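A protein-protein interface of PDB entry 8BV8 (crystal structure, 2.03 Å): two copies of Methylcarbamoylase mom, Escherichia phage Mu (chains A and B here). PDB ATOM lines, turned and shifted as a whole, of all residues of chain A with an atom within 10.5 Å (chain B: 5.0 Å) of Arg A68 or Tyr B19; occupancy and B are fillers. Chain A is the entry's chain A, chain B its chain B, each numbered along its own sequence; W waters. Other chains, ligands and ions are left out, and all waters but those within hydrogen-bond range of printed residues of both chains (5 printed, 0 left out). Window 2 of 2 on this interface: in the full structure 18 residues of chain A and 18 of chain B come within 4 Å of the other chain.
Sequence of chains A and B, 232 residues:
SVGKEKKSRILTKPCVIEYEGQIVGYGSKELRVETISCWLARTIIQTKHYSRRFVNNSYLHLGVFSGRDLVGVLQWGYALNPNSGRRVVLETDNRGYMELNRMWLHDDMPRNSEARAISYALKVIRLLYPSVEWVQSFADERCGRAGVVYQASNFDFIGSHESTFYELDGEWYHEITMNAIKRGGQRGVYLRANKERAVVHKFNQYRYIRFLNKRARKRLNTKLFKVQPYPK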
ATOM      1  N   THR A  12     -40.394   0.583 -28.587  1.00  0.00           N
ATOM      2  CA  THR A  12     -41.176  -0.356 -29.379  1.00  0.00           C
ATOM      3  C   THR A  12     -42.143  -1.107 -28.472  1.00  0.00           C
ATOM      4  O   THR A  12     -42.064  -1.036 -27.243  1.00  0.00           O
ATOM      5  CB  THR A  12     -40.278  -1.343 -30.138  1.00  0.00           C
ATOM      6  OG1 THR A  12     -41.094  -2.277 -30.857  1.00  0.00           O
ATOM      7  CG2 THR A  12     -39.390  -2.100 -29.180  1.00  0.00           C
ATOM      8  N   SER A  28     -39.510  -5.092 -24.221  1.00  0.00           N
ATOM      9  CA  SER A  28     -39.049  -4.704 -25.546  1.00  0.00           C
ATOM     10  C   SER A  28     -37.570  -5.047 -25.699  1.00  0.00           C
ATOM     11  O   SER A  28     -36.914  -5.509 -24.763  1.00  0.00           O
ATOM     12  CB  SER A  28     -39.292  -3.211 -25.772  1.00  0.00           C
ATOM     13  OG  SER A  28     -40.618  -2.853 -25.419  1.00  0.00           O
ATOM     14  N   LYS A  29     -37.038  -4.805 -26.900  1.00  0.00           N
ATOM     15  CA  LYS A  29     -35.616  -5.046 -27.124  1.00  0.00           C
ATOM     16  C   LYS A  29     -34.761  -4.038 -26.367  1.00  0.00           C
ATOM     17  O   LYS A  29     -33.734  -4.402 -25.782  1.00  0.00           O
ATOM     18  CB  LYS A  29     -35.295  -5.011 -28.618  1.00  0.00           C
ATOM     19  CG  LYS A  29     -33.824  -5.273 -28.934  1.00  0.00           C
ATOM     20  CD  LYS A  29     -33.641  -5.853 -30.331  1.00  0.00           C
ATOM     21  CE  LYS A  29     -33.800  -4.794 -31.408  1.00  0.00           C
ATOM     22  NZ  LYS A  29     -32.673  -3.823 -31.395  1.00  0.00           N
ATOM     23  N   GLU A  30     -35.167  -2.765 -26.362  1.00  0.00           N
ATOM     24  CA  GLU A  30     -34.414  -1.748 -25.639  1.00  0.00           C
ATOM     25  C   GLU A  30     -34.631  -1.816 -24.133  1.00  0.00           C
ATOM     26  O   GLU A  30     -33.825  -1.254 -23.383  1.00  0.00           O
ATOM     27  CB  GLU A  30     -34.771  -0.346 -26.142  1.00  0.00           C
ATOM     28  CG  GLU A  30     -36.151   0.142 -25.738  1.00  0.00           C
ATOM     29  CD  GLU A  30     -37.238  -0.362 -26.663  1.00  0.00           C
ATOM     30  OE1 GLU A  30     -36.909  -1.111 -27.605  1.00  0.00           O
ATOM     31  OE2 GLU A  30     -38.416  -0.006 -26.451  1.00  0.00           O
ATOM     32  N   LEU A  31     -35.693  -2.477 -23.676  1.00  0.00           N
ATOM     33  CA  LEU A  31     -35.853  -2.734 -22.249  1.00  0.00           C
ATOM     34  C   LEU A  31     -36.865  -3.847 -22.037  1.00  0.00           C
ATOM     35  O   LEU A  31     -37.985  -3.785 -22.554  1.00  0.00           O
ATOM     36  CB  LEU A  31     -36.286  -1.477 -21.491  1.00  0.00           C
ATOM     37  CG  LEU A  31     -36.085  -1.614 -19.979  1.00  0.00           C
ATOM     38  CD1 LEU A  31     -35.362  -0.403 -19.433  1.00  0.00           C
ATOM     39  CD2 LEU A  31     -37.408  -1.831 -19.257  1.00  0.00           C
ATOM     40  N   ARG A  32     -36.468  -4.853 -21.262  1.00  0.00           N
ATOM     41  CA  ARG A  32     -37.321  -5.983 -20.938  1.00  0.00           C
ATOM     42  C   ARG A  32     -36.845  -6.577 -19.622  1.00  0.00           C
ATOM     43  O   ARG A  32     -35.741  -6.289 -19.152  1.00  0.00           O
ATOM     44  CB  ARG A  32     -37.293  -7.043 -22.043  1.00  0.00           C
ATOM     45  CG  ARG A  32     -35.914  -7.650 -22.257  1.00  0.00           C
ATOM     46  CD  ARG A  32     -35.839  -8.441 -23.552  1.00  0.00           C
ATOM     47  NE  ARG A  32     -34.531  -9.060 -23.727  1.00  0.00           N
ATOM     48  CZ  ARG A  32     -33.480  -8.448 -24.257  1.00  0.00           C
ATOM     49  NH1 ARG A  32     -33.551  -7.198 -24.685  1.00  0.00           N
ATOM     50  NH2 ARG A  32     -32.330  -9.107 -24.356  1.00  0.00           N
ATOM     51  N   GLU A  34     -36.435 -10.424 -17.691  1.00  0.00           N
ATOM     52  CA  GLU A  34     -36.394 -11.865 -17.882  1.00  0.00           C
ATOM     53  C   GLU A  34     -35.900 -12.518 -16.602  1.00  0.00           C
ATOM     54  O   GLU A  34     -35.108 -11.934 -15.858  1.00  0.00           O
ATOM     55  CB  GLU A  34     -35.482 -12.275 -19.050  1.00  0.00           C
ATOM     56  CG  GLU A  34     -35.900 -11.739 -20.411  1.00  0.00           C
ATOM     57  CD  GLU A  34     -35.096 -12.352 -21.542  1.00  0.00           C
ATOM     58  OE1 GLU A  34     -34.589 -13.479 -21.365  1.00  0.00           O
ATOM     59  OE2 GLU A  34     -34.967 -11.706 -22.604  1.00  0.00           O
ATOM     60  N   ILE A  36     -33.701 -14.673 -14.215  1.00  0.00           N
ATOM     61  CA  ILE A  36     -32.297 -15.041 -14.133  1.00  0.00           C
ATOM     62  C   ILE A  36     -32.119 -15.946 -12.920  1.00  0.00           C
ATOM     63  O   ILE A  36     -33.016 -16.093 -12.090  1.00  0.00           O
ATOM     64  CB  ILE A  36     -31.366 -13.815 -14.041  1.00  0.00           C
ATOM     65  CG1 ILE A  36     -31.754 -12.934 -12.851  1.00  0.00           C
ATOM     66  CG2 ILE A  36     -31.401 -13.018 -15.339  1.00  0.00           C
ATOM     67  CD1 ILE A  36     -30.861 -11.726 -12.669  1.00  0.00           C
ATOM     68  N   GLY A  63     -33.713 -10.167 -14.281  1.00  0.00           N
ATOM     69  CA  GLY A  63     -32.716  -9.281 -14.839  1.00  0.00           C
ATOM     70  C   GLY A  63     -33.374  -8.264 -15.754  1.00  0.00           C
ATOM     71  O   GLY A  63     -34.371  -8.552 -16.413  1.00  0.00           O
ATOM     72  N   VAL A  64     -32.818  -7.058 -15.772  1.00  0.00           N
ATOM     73  CA  VAL A  64     -33.256  -6.007 -16.681  1.00  0.00           C
ATOM     74  C   VAL A  64     -32.274  -5.971 -17.842  1.00  0.00           C
ATOM     75  O   VAL A  64     -31.064  -5.820 -17.637  1.00  0.00           O
ATOM     76  CB  VAL A  64     -33.338  -4.646 -15.973  1.00  0.00           C
ATOM     77  CG1 VAL A  64     -33.970  -3.611 -16.890  1.00  0.00           C
ATOM     78  CG2 VAL A  64     -34.125  -4.774 -14.679  1.00  0.00           C
ATOM     79  N   PHE A  65     -32.787  -6.124 -19.058  1.00  0.00           N
ATOM     80  CA  PHE A  65     -31.957  -6.212 -20.248  1.00  0.00           C
ATOM     81  C   PHE A  65     -32.259  -5.058 -21.193  1.00  0.00           C
ATOM     82  O   PHE A  65     -33.413  -4.646 -21.342  1.00  0.00           O
ATOM     83  CB  PHE A  65     -32.169  -7.547 -20.968  1.00  0.00           C
ATOM     84  CG  PHE A  65     -31.734  -8.744 -20.166  1.00  0.00           C
ATOM     85  CD1 PHE A  65     -32.623  -9.395 -19.325  1.00  0.00           C
ATOM     86  CD2 PHE A  65     -30.433  -9.216 -20.254  1.00  0.00           C
ATOM     87  CE1 PHE A  65     -32.224 -10.498 -18.587  1.00  0.00           C
ATOM     88  CE2 PHE A  65     -30.026 -10.319 -19.518  1.00  0.00           C
ATOM     89  CZ  PHE A  65     -30.921 -10.960 -18.684  1.00  0.00           C
ATOM     90  N   SER A  66     -31.209  -4.544 -21.828  1.00  0.00           N
ATOM     91  CA  SER A  66     -31.316  -3.503 -22.845  1.00  0.00           C
ATOM     92  C   SER A  66     -30.461  -3.930 -24.030  1.00  0.00           C
ATOM     93  O   SER A  66     -29.229  -3.908 -23.949  1.00  0.00           O
ATOM     94  CB  SER A  66     -30.869  -2.147 -22.301  1.00  0.00           C
ATOM     95  OG  SER A  66     -31.030  -1.132 -23.276  1.00  0.00           O
ATOM     96  N   GLY A  67     -31.111  -4.319 -25.123  1.00  0.00           N
ATOM     97  CA  GLY A  67     -30.401  -4.951 -26.216  1.00  0.00           C
ATOM     98  C   GLY A  67     -29.956  -6.344 -25.823  1.00  0.00           C
ATOM     99  O   GLY A  67     -30.790  -7.203 -25.522  1.00  0.00           O
ATOM    100  N   ARG A  68     -28.646  -6.581 -25.809  1.00  0.00           N
ATOM    101  CA  ARG A  68     -28.088  -7.842 -25.340  1.00  0.00           C
ATOM    102  C   ARG A  68     -27.425  -7.709 -23.977  1.00  0.00           C
ATOM    103  O   ARG A  68     -26.790  -8.662 -23.512  1.00  0.00           O
ATOM    104  CB  ARG A  68     -27.086  -8.391 -26.359  1.00  0.00           C
ATOM    105  CG  ARG A  68     -25.864  -7.508 -26.565  1.00  0.00           C
ATOM    106  CD  ARG A  68     -24.878  -8.138 -27.538  1.00  0.00           C
ATOM    107  NE  ARG A  68     -24.290  -9.363 -27.008  1.00  0.00           N
ATOM    108  CZ  ARG A  68     -23.152  -9.415 -26.327  1.00  0.00           C
ATOM    109  NH1 ARG A  68     -22.450  -8.323 -26.071  1.00  0.00           N
ATOM    110  NH2 ARG A  68     -22.708 -10.591 -25.895  1.00  0.00           N
ATOM    111  N   ASP A  69     -27.566  -6.560 -23.323  1.00  0.00           N
ATOM    112  CA  ASP A  69     -26.833  -6.253 -22.102  1.00  0.00           C
ATOM    113  C   ASP A  69     -27.740  -6.374 -20.884  1.00  0.00           C
ATOM    114  O   ASP A  69     -28.862  -5.857 -20.884  1.00  0.00           O
ATOM    115  CB  ASP A  69     -26.242  -4.844 -22.169  1.00  0.00           C
ATOM    116  CG  ASP A  69     -25.263  -4.677 -23.312  1.00  0.00           C
ATOM    117  OD1 ASP A  69     -24.485  -5.619 -23.572  1.00  0.00           O
ATOM    118  OD2 ASP A  69     -25.269  -3.602 -23.948  1.00  0.00           O
ATOM    119  N   LEU A  70     -27.245  -7.053 -19.851  1.00  0.00           N
ATOM    120  CA  LEU A  70     -27.891  -7.063 -18.545  1.00  0.00           C
ATOM    121  C   LEU A  70     -27.548  -5.767 -17.821  1.00  0.00           C
ATOM    122  O   LEU A  70     -26.368  -5.446 -17.646  1.00  0.00           O
ATOM    123  CB  LEU A  70     -27.430  -8.277 -17.741  1.00  0.00           C
ATOM    124  CG  LEU A  70     -27.829  -8.373 -16.268  1.00  0.00           C
ATOM    125  CD1 LEU A  70     -29.332  -8.515 -16.122  1.00  0.00           C
ATOM    126  CD2 LEU A  70     -27.109  -9.538 -15.606  1.00  0.00           C
ATOM    127  N   VAL A  71     -28.569  -5.011 -17.413  1.00  0.00           N
ATOM    128  CA  VAL A  71     -28.340  -3.664 -16.897  1.00  0.00           C
ATOM    129  C   VAL A  71     -29.047  -3.438 -15.566  1.00  0.00           C
ATOM    130  O   VAL A  71     -29.053  -2.317 -15.047  1.00  0.00           O
ATOM    131  CB  VAL A  71     -28.778  -2.596 -17.919  1.00  0.00           C
ATOM    132  CG1 VAL A  71     -28.017  -2.750 -19.230  1.00  0.00           C
ATOM    133  CG2 VAL A  71     -30.281  -2.661 -18.154  1.00  0.00           C
ATOM    134  N   GLY A  72     -29.646  -4.479 -14.999  1.00  0.00           N
ATOM    135  CA  GLY A  72     -30.346  -4.298 -13.740  1.00  0.00           C
ATOM    136  C   GLY A  72     -30.899  -5.603 -13.213  1.00  0.00           C
ATOM    137  O   GLY A  72     -30.904  -6.630 -13.899  1.00  0.00           O
ATOM    138  N   MET A 109     -28.422   4.039 -17.334  1.00  0.00           N
ATOM    139  CA  MET A 109     -29.698   3.789 -17.982  1.00  0.00           C
ATOM    140  C   MET A 109     -30.572   5.042 -17.945  1.00  0.00           C
ATOM    141  O   MET A 109     -30.452   5.862 -17.029  1.00  0.00           O
ATOM    142  CB  MET A 109     -30.425   2.635 -17.301  1.00  0.00           C
ATOM    143  CG  MET A 109     -29.803   1.272 -17.557  1.00  0.00           C
ATOM    144  SD  MET A 109     -29.826   0.819 -19.303  1.00  0.00           S
ATOM    145  CE  MET A 109     -31.588   0.732 -19.612  1.00  0.00           C
ATOM    146  N   ILE B  17     -20.715 -16.011 -33.174  1.00  0.00           N
ATOM    147  CA  ILE B  17     -21.993 -15.485 -32.712  1.00  0.00           C
ATOM    148  C   ILE B  17     -22.001 -13.979 -32.928  1.00  0.00           C
ATOM    149  O   ILE B  17     -21.098 -13.273 -32.463  1.00  0.00           O
ATOM    150  CB  ILE B  17     -22.239 -15.837 -31.236  1.00  0.00           C
ATOM    151  CG1 ILE B  17     -22.272 -17.356 -31.068  1.00  0.00           C
ATOM    152  CG2 ILE B  17     -23.534 -15.208 -30.743  1.00  0.00           C
ATOM    153  CD1 ILE B  17     -22.021 -17.816 -29.662  1.00  0.00           C
ATOM    154  N   GLU B  18     -23.022 -13.491 -33.625  1.00  0.00           N
ATOM    155  CA  GLU B  18     -23.129 -12.091 -33.995  1.00  0.00           C
ATOM    156  C   GLU B  18     -24.371 -11.466 -33.376  1.00  0.00           C
ATOM    157  O   GLU B  18     -25.351 -12.153 -33.071  1.00  0.00           O
ATOM    158  CB  GLU B  18     -23.176 -11.926 -35.521  1.00  0.00           C
ATOM    159  CG  GLU B  18     -21.895 -12.331 -36.234  1.00  0.00           C
ATOM    160  CD  GLU B  18     -22.065 -12.403 -37.740  1.00  0.00           C
ATOM    161  OE1 GLU B  18     -22.899 -13.208 -38.206  1.00  0.00           O
ATOM    162  OE2 GLU B  18     -21.372 -11.652 -38.458  1.00  0.00           O
ATOM    163  N   TYR B  19     -24.313 -10.150 -33.187  1.00  0.00           N
ATOM    164  CA  TYR B  19     -25.459  -9.364 -32.739  1.00  0.00           C
ATOM    165  C   TYR B  19     -25.435  -8.047 -33.502  1.00  0.00           C
ATOM    166  O   TYR B  19     -24.509  -7.248 -33.327  1.00  0.00           O
ATOM    167  CB  TYR B  19     -25.427  -9.126 -31.230  1.00  0.00           C
ATOM    168  CG  TYR B  19     -26.682  -8.473 -30.694  1.00  0.00           C
ATOM    169  CD1 TYR B  19     -27.793  -9.236 -30.359  1.00  0.00           C
ATOM    170  CD2 TYR B  19     -26.757  -7.097 -30.527  1.00  0.00           C
ATOM    171  CE1 TYR B  19     -28.946  -8.645 -29.871  1.00  0.00           C
ATOM    172  CE2 TYR B  19     -27.905  -6.498 -30.040  1.00  0.00           C
ATOM    173  CZ  TYR B  19     -28.996  -7.277 -29.713  1.00  0.00           C
ATOM    174  OH  TYR B  19     -30.140  -6.684 -29.227  1.00  0.00           O
ATOM    175  N   GLU B  20     -26.445  -7.831 -34.347  1.00  0.00           N
ATOM    176  CA  GLU B  20     -26.513  -6.659 -35.221  1.00  0.00           C
ATOM    177  C   GLU B  20     -25.278  -6.573 -36.117  1.00  0.00           C
ATOM    178  O   GLU B  20     -24.650  -5.522 -36.255  1.00  0.00           O
ATOM    179  CB  GLU B  20     -26.701  -5.372 -34.413  1.00  0.00           C
ATOM    180  CG  GLU B  20     -27.998  -5.316 -33.626  1.00  0.00           C
ATOM    181  CD  GLU B  20     -28.127  -4.051 -32.804  1.00  0.00           C
ATOM    182  OE1 GLU B  20     -27.160  -3.260 -32.771  1.00  0.00           O
ATOM    183  OE2 GLU B  20     -29.195  -3.846 -32.190  1.00  0.00           O
ATOM    184  N   GLY B  21     -24.926  -7.706 -36.723  1.00  0.00           N
ATOM    185  CA  GLY B  21     -23.802  -7.767 -37.637  1.00  0.00           C
ATOM    186  C   GLY B  21     -22.451  -7.894 -36.962  1.00  0.00           C
ATOM    187  O   GLY B  21     -21.534  -8.511 -37.512  1.00  0.00           O
ATOM    188  N   GLN B  22     -22.315  -7.322 -35.768  1.00  0.00           N
ATOM    189  CA  GLN B  22     -21.032  -7.296 -35.081  1.00  0.00           C
ATOM    190  C   GLN B  22     -20.728  -8.641 -34.430  1.00  0.00           C
ATOM    191  O   GLN B  22     -21.619  -9.305 -33.894  1.00  0.00           O
ATOM    192  CB  GLN B  22     -21.020  -6.190 -34.026  1.00  0.00           C
ATOM    193  CG  GLN B  22     -21.259  -4.802 -34.592  1.00  0.00           C
ATOM    194  CD  GLN B  22     -20.916  -3.703 -33.607  1.00  0.00           C
ATOM    195  OE1 GLN B  22     -20.642  -3.968 -32.437  1.00  0.00           O
ATOM    196  NE2 GLN B  22     -20.924  -2.462 -34.078  1.00  0.00           N
ATOM    197  N   VAL B  24     -19.606 -11.065 -31.650  1.00  0.00           N
ATOM    198  CA  VAL B  24     -19.840 -10.913 -30.220  1.00  0.00           C
ATOM    199  C   VAL B  24     -19.309 -12.110 -29.433  1.00  0.00           C
ATOM    200  O   VAL B  24     -18.944 -11.976 -28.261  1.00  0.00           O
ATOM    201  CB  VAL B  24     -21.340 -10.676 -29.947  1.00  0.00           C
ATOM    202  CG1 VAL B  24     -21.921 -11.733 -29.013  1.00  0.00           C
ATOM    203  CG2 VAL B  24     -21.560  -9.277 -29.388  1.00  0.00           C
ATOM    204  N   GLU B  34     -19.383 -15.127 -24.819  1.00  0.00           N
ATOM    205  CA  GLU B  34     -19.721 -13.862 -25.454  1.00  0.00           C
ATOM    206  C   GLU B  34     -19.178 -12.725 -24.603  1.00  0.00           C
ATOM    207  O   GLU B  34     -18.921 -12.887 -23.408  1.00  0.00           O
ATOM    208  CB  GLU B  34     -21.239 -13.699 -25.642  1.00  0.00           C
ATOM    209  CG  GLU B  34     -21.918 -14.832 -26.400  1.00  0.00           C
ATOM    210  CD  GLU B  34     -23.383 -14.550 -26.676  1.00  0.00           C
ATOM    211  OE1 GLU B  34     -23.748 -13.362 -26.813  1.00  0.00           O
ATOM    212  OE2 GLU B  34     -24.172 -15.514 -26.752  1.00  0.00           O
ATOM    213  N   THR B  35     -19.004 -11.567 -25.233  1.00  0.00           N
ATOM    214  CA  THR B  35     -18.552 -10.392 -24.502  1.00  0.00           C
ATOM    215  C   THR B  35     -19.627  -9.919 -23.532  1.00  0.00           C
ATOM    216  O   THR B  35     -20.821  -9.936 -23.843  1.00  0.00           O
ATOM    217  CB  THR B  35     -18.193  -9.258 -25.466  1.00  0.00           C
ATOM    218  OG1 THR B  35     -19.289  -9.020 -26.358  1.00  0.00           O
ATOM    219  CG2 THR B  35     -16.950  -9.610 -26.269  1.00  0.00           C
HETATM  220  O   HOH W   1     -24.167  -9.712 -22.887  1.00  0.00           O
HETATM  221  O   HOH W   2     -20.701  -6.464 -24.005  1.00  0.00           O
HETATM  222  O   HOH W   3     -31.152  -5.999 -33.165  1.00  0.00           O
HETATM  223  O   HOH W   4     -30.067  -4.002 -29.696  1.00  0.00           O
HETATM  224  O   HOH W   5     -25.785 -11.920 -27.881  1.00  0.00           O
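Among the printed residues, pairs that only touch across the chains: Arg A68 with Val B24, Gly A67 with Tyr B19, Arg A68 with Tyr B19 and Lys A29 with Tyr B19.
1 position is printed for both chains. Of the 7 pairs that touch across the chains among the printed residues, none has its exchanged pair printed and touching as well.
The guanidinium group (NH1) of Arg A32 sits at hydrogen-bond distance from the backbone carbonyl oxygen (O) of Lys A29 (3.0 Å). The backbone NH of Gly A67 is in hydrogen-bond range of the backbone carbonyl oxygen of Lys A29 (2.7 Å). O of Val B24 sits at hydrogen-bond distance from N of Thr B35 (3.1 Å). The backbone carbonyl oxygen (O) of Ile B17 lies within hydrogen-bond range of the backbone NH (N) of Val B24. The guanidinium group of Arg A32 sits at hydrogen-bond distance from the backbone carbonyl oxygen of Gly A67 (2.7 Å).
Along chain A the printed residues that touch a printed residue of chain B span positions 29 to 68. Of the 9 printed residues of chain B, 5 touch a printed residue of chain A. Hydrophobic or aromatic side chains of chain B that line the printed part of chain A: Tyr B19 and Val B24. Among the printed residues, Asp or Glu carboxylates within 4 Å of a Lys or Arg side-chain nitrogen of the other chain: Lys A29 with Glu B20 (3.6 Å) and Arg A68 with Glu B34 (3.1 Å).
Water W4 lies within hydrogen-bond range of the side-chain carboxylate of Glu B20 (2.6 Å), the side-chain hydroxyl of Tyr B19 (2.7 Å) and the side-chain amino group of Lys A29 (3.1 Å). Water W5 bridges OE1 of Glu B34 (2.7 Å) and NE of Arg A68 (3.1 Å). Water W1 lies within hydrogen-bond range of O of Arg A68 (2.9 Å) and O of Thr B35 (3.5 Å). Water W3 bridges the side-chain carboxylate of Glu B20 and the side-chain amino group of Lys A29. Water W2 lies within hydrogen-bond range of NH1 of Arg A68 (3.3 Å) and O of Thr B35 (3.5 Å).
The guanidinium group (NH2) of Arg A68 is in hydrogen-bond range of the backbone carbonyl oxygen (O) of Thr B35, at 2.9 Å. The side-chain amino group of Lys A29 lies within salt-bridge range of the side-chain carboxylate of Glu B20, at 3.6 Å. The guanidinium group (NH2) of Arg A68 is in salt-bridge range of the side-chain carboxylate (OE1) of Glu B34, 3.1 Å away.
Arg A68 touches four residues of chain B. Of chain A, only Lys A29, Gly A67 and Arg A68 come within 4 Å of Tyr B19. Of chain A, only Lys A29 (3.6 Å) comes within 4 Å of Glu B20. Gly B21 touches none of the printed residues of chain A. Gln B22 touches none of the printed residues of chain A. Of the printed residues of chain A, Glu B34 touches Arg A68. Of the printed residues of chain B, Lys A29 touches Tyr B19 (3.8 Å) and Glu B20 (3.6 Å). Of the printed residues of chain B, Gly A67 touches Tyr B19.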
